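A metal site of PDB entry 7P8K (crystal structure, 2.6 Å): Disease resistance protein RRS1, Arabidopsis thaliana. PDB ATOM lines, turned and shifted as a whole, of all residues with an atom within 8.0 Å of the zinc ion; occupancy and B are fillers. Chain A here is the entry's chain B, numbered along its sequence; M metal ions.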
ATOM      1  N   TRP A  20      -1.867 -18.598 -15.616  1.00  0.00           N
ATOM      2  CA  TRP A  20      -1.453 -17.395 -16.406  1.00  0.00           C
ATOM      3  C   TRP A  20      -0.124 -16.846 -15.868  1.00  0.00           C
ATOM      4  O   TRP A  20       0.290 -17.252 -14.762  1.00  0.00           O
ATOM      5  CB  TRP A  20      -2.552 -16.320 -16.394  1.00  0.00           C
ATOM      6  CG  TRP A  20      -3.887 -16.803 -16.864  1.00  0.00           C
ATOM      7  CD1 TRP A  20      -4.937 -17.223 -16.098  1.00  0.00           C
ATOM      8  CD2 TRP A  20      -4.326 -16.904 -18.231  1.00  0.00           C
ATOM      9  NE1 TRP A  20      -5.992 -17.607 -16.877  1.00  0.00           N
ATOM     10  CE2 TRP A  20      -5.645 -17.413 -18.199  1.00  0.00           C
ATOM     11  CE3 TRP A  20      -3.744 -16.629 -19.465  1.00  0.00           C
ATOM     12  CZ2 TRP A  20      -6.383 -17.648 -19.355  1.00  0.00           C
ATOM     13  CZ3 TRP A  20      -4.474 -16.862 -20.617  1.00  0.00           C
ATOM     14  CH2 TRP A  20      -5.772 -17.364 -20.562  1.00  0.00           C
ATOM     15  N   THR A  21       0.516 -15.949 -16.632  1.00  0.00           N
ATOM     16  CA  THR A  21       1.729 -15.185 -16.217  1.00  0.00           C
ATOM     17  C   THR A  21       1.313 -13.736 -15.941  1.00  0.00           C
ATOM     18  O   THR A  21       0.645 -13.137 -16.793  1.00  0.00           O
ATOM     19  CB  THR A  21       2.846 -15.275 -17.261  1.00  0.00           C
ATOM     20  OG1 THR A  21       2.305 -15.161 -18.580  1.00  0.00           O
ATOM     21  CG2 THR A  21       3.635 -16.559 -17.162  1.00  0.00           C
ATOM     22  N   TRP A  22       1.721 -13.220 -14.775  1.00  0.00           N
ATOM     23  CA  TRP A  22       1.306 -11.903 -14.220  1.00  0.00           C
ATOM     24  C   TRP A  22       2.530 -11.010 -13.972  1.00  0.00           C
ATOM     25  O   TRP A  22       3.634 -11.543 -13.834  1.00  0.00           O
ATOM     26  CB  TRP A  22       0.531 -12.127 -12.931  1.00  0.00           C
ATOM     27  CG  TRP A  22      -0.640 -13.037 -13.099  1.00  0.00           C
ATOM     28  CD1 TRP A  22      -0.688 -14.374 -12.822  1.00  0.00           C
ATOM     29  CD2 TRP A  22      -1.932 -12.675 -13.609  1.00  0.00           C
ATOM     30  NE1 TRP A  22      -1.927 -14.867 -13.120  1.00  0.00           N
ATOM     31  CE2 TRP A  22      -2.716 -13.846 -13.596  1.00  0.00           C
ATOM     32  CE3 TRP A  22      -2.504 -11.488 -14.068  1.00  0.00           C
ATOM     33  CZ2 TRP A  22      -4.038 -13.853 -14.029  1.00  0.00           C
ATOM     34  CZ3 TRP A  22      -3.809 -11.491 -14.492  1.00  0.00           C
ATOM     35  CH2 TRP A  22      -4.571 -12.658 -14.479  1.00  0.00           C
ATOM     36  N   ARG A  41      -1.462  -7.470 -13.348  1.00  0.00           N
ATOM     37  CA  ARG A  41      -1.901  -7.356 -14.771  1.00  0.00           C
ATOM     38  C   ARG A  41      -1.177  -8.419 -15.607  1.00  0.00           C
ATOM     39  O   ARG A  41      -0.071  -8.805 -15.235  1.00  0.00           O
ATOM     40  CB  ARG A  41      -1.667  -5.958 -15.335  1.00  0.00           C
ATOM     41  CG  ARG A  41      -0.255  -5.412 -15.168  1.00  0.00           C
ATOM     42  CD  ARG A  41       0.719  -5.894 -16.220  1.00  0.00           C
ATOM     43  NE  ARG A  41       1.793  -4.926 -16.419  1.00  0.00           N
ATOM     44  CZ  ARG A  41       2.953  -5.176 -17.015  1.00  0.00           C
ATOM     45  NH1 ARG A  41       3.221  -6.381 -17.498  1.00  0.00           N
ATOM     46  NH2 ARG A  41       3.854  -4.211 -17.128  1.00  0.00           N
ATOM     47  N   CYS A  42      -1.786  -8.855 -16.715  1.00  0.00           N
ATOM     48  CA  CYS A  42      -1.247  -9.953 -17.559  1.00  0.00           C
ATOM     49  C   CYS A  42       0.140  -9.543 -18.060  1.00  0.00           C
ATOM     50  O   CYS A  42       0.333  -8.363 -18.427  1.00  0.00           O
ATOM     51  CB  CYS A  42      -2.163 -10.277 -18.733  1.00  0.00           C
ATOM     52  SG  CYS A  42      -1.618 -11.729 -19.681  1.00  0.00           S
ATOM     53  N   ALA A  43       1.086 -10.491 -18.064  1.00  0.00           N
ATOM     54  CA  ALA A  43       2.446 -10.310 -18.603  1.00  0.00           C
ATOM     55  C   ALA A  43       2.345  -9.842 -20.063  1.00  0.00           C
ATOM     56  O   ALA A  43       3.289  -9.193 -20.542  1.00  0.00           O
ATOM     57  CB  ALA A  43       3.229 -11.588 -18.474  1.00  0.00           C
ATOM     58  N   TYR A  44       1.223 -10.157 -20.728  1.00  0.00           N
ATOM     59  CA  TYR A  44       1.012  -9.908 -22.182  1.00  0.00           C
ATOM     60  C   TYR A  44       0.199  -8.631 -22.386  1.00  0.00           C
ATOM     61  O   TYR A  44      -0.205  -8.357 -23.536  1.00  0.00           O
ATOM     62  CB  TYR A  44       0.353 -11.138 -22.809  1.00  0.00           C
ATOM     63  CG  TYR A  44       1.204 -12.380 -22.693  1.00  0.00           C
ATOM     64  CD1 TYR A  44       2.399 -12.495 -23.396  1.00  0.00           C
ATOM     65  CD2 TYR A  44       0.844 -13.422 -21.862  1.00  0.00           C
ATOM     66  CE1 TYR A  44       3.189 -13.612 -23.289  1.00  0.00           C
ATOM     67  CE2 TYR A  44       1.625 -14.546 -21.736  1.00  0.00           C
ATOM     68  CZ  TYR A  44       2.809 -14.645 -22.448  1.00  0.00           C
ATOM     69  OH  TYR A  44       3.585 -15.762 -22.337  1.00  0.00           O
ATOM     70  N   LYS A  45       0.002  -7.851 -21.319  1.00  0.00           N
ATOM     71  CA  LYS A  45      -0.762  -6.570 -21.355  1.00  0.00           C
ATOM     72  C   LYS A  45      -0.271  -5.725 -22.534  1.00  0.00           C
ATOM     73  O   LYS A  45      -1.108  -5.144 -23.236  1.00  0.00           O
ATOM     74  CB  LYS A  45      -0.601  -5.821 -20.031  1.00  0.00           C
ATOM     75  CG  LYS A  45      -1.263  -4.449 -19.953  1.00  0.00           C
ATOM     76  CD  LYS A  45      -0.956  -3.746 -18.642  1.00  0.00           C
ATOM     77  CE  LYS A  45      -1.396  -2.298 -18.623  1.00  0.00           C
ATOM     78  NZ  LYS A  45      -2.871  -2.180 -18.745  1.00  0.00           N
ATOM     79  N   HIS A  48       0.505  -8.136 -26.329  1.00  0.00           N
ATOM     80  CA  HIS A  48      -0.733  -8.701 -26.941  1.00  0.00           C
ATOM     81  C   HIS A  48      -1.961  -7.801 -26.672  1.00  0.00           C
ATOM     82  O   HIS A  48      -3.036  -8.120 -27.205  1.00  0.00           O
ATOM     83  CB  HIS A  48      -0.985 -10.122 -26.419  1.00  0.00           C
ATOM     84  CG  HIS A  48       0.064 -11.114 -26.810  1.00  0.00           C
ATOM     85  ND1 HIS A  48       1.407 -10.906 -26.595  1.00  0.00           N
ATOM     86  CD2 HIS A  48      -0.032 -12.343 -27.382  1.00  0.00           C
ATOM     87  CE1 HIS A  48       2.094 -11.943 -27.025  1.00  0.00           C
ATOM     88  NE2 HIS A  48       1.243 -12.844 -27.512  1.00  0.00           N
ATOM     89  N   GLY A  49      -1.809  -6.733 -25.892  1.00  0.00           N
ATOM     90  CA  GLY A  49      -2.897  -5.776 -25.586  1.00  0.00           C
ATOM     91  C   GLY A  49      -3.855  -6.303 -24.529  1.00  0.00           C
ATOM     92  O   GLY A  49      -4.957  -5.741 -24.402  1.00  0.00           O
ATOM     93  N   CYS A  50      -3.473  -7.345 -23.783  1.00  0.00           N
ATOM     94  CA  CYS A  50      -4.341  -8.056 -22.807  1.00  0.00           C
ATOM     95  C   CYS A  50      -4.859  -7.068 -21.736  1.00  0.00           C
ATOM     96  O   CYS A  50      -4.079  -6.212 -21.271  1.00  0.00           O
ATOM     97  CB  CYS A  50      -3.592  -9.221 -22.169  1.00  0.00           C
ATOM     98  SG  CYS A  50      -4.702 -10.420 -21.383  1.00  0.00           S
ATOM     99  N   LYS A  51      -6.144  -7.190 -21.385  1.00  0.00           N
ATOM    100  CA  LYS A  51      -6.853  -6.304 -20.431  1.00  0.00           C
ATOM    101  C   LYS A  51      -6.881  -6.948 -19.040  1.00  0.00           C
ATOM    102  O   LYS A  51      -7.078  -6.219 -18.058  1.00  0.00           O
ATOM    103  CB  LYS A  51      -8.307  -6.069 -20.862  1.00  0.00           C
ATOM    104  CG  LYS A  51      -8.528  -5.010 -21.937  1.00  0.00           C
ATOM    105  CD  LYS A  51      -9.858  -5.194 -22.686  1.00  0.00           C
ATOM    106  CE  LYS A  51     -11.063  -5.394 -21.775  1.00  0.00           C
ATOM    107  NZ  LYS A  51     -12.284  -5.717 -22.555  1.00  0.00           N
ATOM    108  N   ALA A  52      -6.703  -8.275 -18.973  1.00  0.00           N
ATOM    109  CA  ALA A  52      -6.932  -9.125 -17.782  1.00  0.00           C
ATOM    110  C   ALA A  52      -6.129  -8.597 -16.600  1.00  0.00           C
ATOM    111  O   ALA A  52      -4.965  -8.177 -16.800  1.00  0.00           O
ATOM    112  CB  ALA A  52      -6.568 -10.550 -18.104  1.00  0.00           C
ATOM    113  N   THR A  53      -6.723  -8.635 -15.410  1.00  0.00           N
ATOM    114  CA  THR A  53      -6.102  -8.288 -14.107  1.00  0.00           C
ATOM    115  C   THR A  53      -6.661  -9.215 -13.024  1.00  0.00           C
ATOM    116  O   THR A  53      -7.725  -9.824 -13.248  1.00  0.00           O
ATOM    117  CB  THR A  53      -6.342  -6.821 -13.755  1.00  0.00           C
ATOM    118  OG1 THR A  53      -7.742  -6.575 -13.901  1.00  0.00           O
ATOM    119  CG2 THR A  53      -5.559  -5.867 -14.619  1.00  0.00           C
ATOM    120  N   SER A  72     -11.761  -9.311 -16.141  1.00  0.00           N
ATOM    121  CA  SER A  72     -11.572  -9.392 -17.627  1.00  0.00           C
ATOM    122  C   SER A  72     -10.882 -10.700 -18.025  1.00  0.00           C
ATOM    123  O   SER A  72      -9.920 -11.084 -17.387  1.00  0.00           O
ATOM    124  CB  SER A  72     -10.815  -8.210 -18.158  1.00  0.00           C
ATOM    125  OG  SER A  72     -11.498  -7.001 -17.835  1.00  0.00           O
ATOM    126  N   GLU A  73     -11.359 -11.327 -19.097  1.00  0.00           N
ATOM    127  CA  GLU A  73     -10.757 -12.553 -19.674  1.00  0.00           C
ATOM    128  C   GLU A  73      -9.533 -12.136 -20.503  1.00  0.00           C
ATOM    129  O   GLU A  73      -9.440 -10.950 -20.881  1.00  0.00           O
ATOM    130  CB  GLU A  73     -11.808 -13.291 -20.511  1.00  0.00           C
ATOM    131  CG  GLU A  73     -11.744 -14.800 -20.364  1.00  0.00           C
ATOM    132  CD  GLU A  73     -13.110 -15.459 -20.370  1.00  0.00           C
ATOM    133  OE1 GLU A  73     -13.583 -15.842 -19.266  1.00  0.00           O
ATOM    134  OE2 GLU A  73     -13.695 -15.576 -21.457  1.00  0.00           O
ATOM    135  N   HIS A  74      -8.617 -13.072 -20.759  1.00  0.00           N
ATOM    136  CA  HIS A  74      -7.382 -12.845 -21.564  1.00  0.00           C
ATOM    137  C   HIS A  74      -7.727 -12.879 -23.050  1.00  0.00           C
ATOM    138  O   HIS A  74      -8.638 -13.624 -23.409  1.00  0.00           O
ATOM    139  CB  HIS A  74      -6.306 -13.887 -21.245  1.00  0.00           C
ATOM    140  CG  HIS A  74      -5.771 -13.800 -19.857  1.00  0.00           C
ATOM    141  ND1 HIS A  74      -4.587 -13.161 -19.567  1.00  0.00           N
ATOM    142  CD2 HIS A  74      -6.241 -14.292 -18.687  1.00  0.00           C
ATOM    143  CE1 HIS A  74      -4.356 -13.246 -18.268  1.00  0.00           C
ATOM    144  NE2 HIS A  74      -5.356 -13.935 -17.709  1.00  0.00           N
ATOM    145  N   ASN A  75      -6.998 -12.105 -23.859  1.00  0.00           N
ATOM    146  CA  ASN A  75      -7.131 -12.070 -25.338  1.00  0.00           C
ATOM    147  C   ASN A  75      -6.012 -12.923 -25.969  1.00  0.00           C
ATOM    148  O   ASN A  75      -5.425 -12.498 -27.002  1.00  0.00           O
ATOM    149  CB  ASN A  75      -7.138 -10.640 -25.860  1.00  0.00           C
ATOM    150  CG  ASN A  75      -5.796  -9.971 -25.706  1.00  0.00           C
ATOM    151  OD1 ASN A  75      -4.987 -10.396 -24.893  1.00  0.00           O
ATOM    152  ND2 ASN A  75      -5.554  -8.932 -26.488  1.00  0.00           N
ATOM    153  N   HIS A  76      -5.760 -14.102 -25.392  1.00  0.00           N
ATOM    154  CA  HIS A  76      -4.730 -15.070 -25.846  1.00  0.00           C
ATOM    155  C   HIS A  76      -4.920 -16.371 -25.062  1.00  0.00           C
ATOM    156  O   HIS A  76      -5.577 -16.371 -24.031  1.00  0.00           O
ATOM    157  CB  HIS A  76      -3.328 -14.484 -25.679  1.00  0.00           C
ATOM    158  CG  HIS A  76      -3.064 -13.979 -24.303  1.00  0.00           C
ATOM    159  ND1 HIS A  76      -2.731 -14.822 -23.255  1.00  0.00           N
ATOM    160  CD2 HIS A  76      -3.110 -12.727 -23.782  1.00  0.00           C
ATOM    161  CE1 HIS A  76      -2.582 -14.105 -22.154  1.00  0.00           C
ATOM    162  NE2 HIS A  76      -2.806 -12.819 -22.463  1.00  0.00           N
ATOM    163  N   PRO A  77      -4.372 -17.507 -25.534  1.00  0.00           N
ATOM    164  CA  PRO A  77      -4.381 -18.743 -24.749  1.00  0.00           C
ATOM    165  C   PRO A  77      -3.325 -18.646 -23.644  1.00  0.00           C
ATOM    166  O   PRO A  77      -2.469 -17.788 -23.753  1.00  0.00           O
ATOM    167  CB  PRO A  77      -4.007 -19.812 -25.774  1.00  0.00           C
ATOM    168  CG  PRO A  77      -3.081 -19.066 -26.721  1.00  0.00           C
ATOM    169  CD  PRO A  77      -3.659 -17.670 -26.810  1.00  0.00           C
ATOM    170  N   ARG A  78      -3.403 -19.506 -22.622  1.00  0.00           N
ATOM    171  CA  ARG A  78      -2.372 -19.554 -21.555  1.00  0.00           C
ATOM    172  C   ARG A  78      -1.117 -20.176 -22.155  1.00  0.00           C
ATOM    173  O   ARG A  78      -1.218 -21.067 -23.004  1.00  0.00           O
ATOM    174  CB  ARG A  78      -2.846 -20.279 -20.269  1.00  0.00           C
ATOM    175  CG  ARG A  78      -4.009 -21.246 -20.424  1.00  0.00           C
ATOM    176  CD  ARG A  78      -3.642 -22.533 -21.139  1.00  0.00           C
ATOM    177  NE  ARG A  78      -4.569 -23.619 -20.813  1.00  0.00           N
ATOM    178  CZ  ARG A  78      -4.444 -24.885 -21.216  1.00  0.00           C
ATOM    179  NH1 ARG A  78      -3.422 -25.243 -21.981  1.00  0.00           N
ATOM    180  NH2 ARG A  78      -5.342 -25.783 -20.857  1.00  0.00           N
ATOM    181  N   PRO A  79       0.092 -19.703 -21.790  1.00  0.00           N
ATOM    182  CA  PRO A  79       1.334 -20.158 -22.424  1.00  0.00           C
ATOM    183  C   PRO A  79       1.952 -21.365 -21.715  1.00  0.00           C
ATOM    184  O   PRO A  79       1.539 -21.659 -20.613  1.00  0.00           O
ATOM    185  CB  PRO A  79       2.212 -18.909 -22.279  1.00  0.00           C
ATOM    186  CG  PRO A  79       1.831 -18.372 -20.907  1.00  0.00           C
ATOM    187  CD  PRO A  79       0.353 -18.697 -20.751  1.00  0.00           C
HETATM  188 ZN    ZN M   1      -3.503 -12.228 -20.593  1.00  0.00          ZN
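The backbone NH of Cys 42 sits at hydrogen-bond distance from the backbone carbonyl oxygen of Ala 52, 3.3 Å away.
N of Tyr 44 sits close to SG of Cys 42 (3.4 Å).
N of Ala 52 sits close to SG of Cys 50, 3.8 Å away.
N of Cys 50 lies within hydrogen-bond range of O of Tyr 44, 3.4 Å away.
OD1 of Asn 75 sits close to SG of Cys 50, at 3.5 Å.
O of Lys 45 lies within hydrogen-bond range of N of Cys 50 (3.3 Å).
Of the 22 residues printed, 4 come within 4 Å of the zinc ion.
The zinc ion is bound by a ring nitrogen (ND1) of His 74 (1.8 Å), a ring nitrogen (NE2) of His 76 (2.1 Å), the side-chain sulfur (SG) of Cys 42 (2.2 Å) and the side-chain sulfur (SG) of Cys 50 (2.3 Å).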
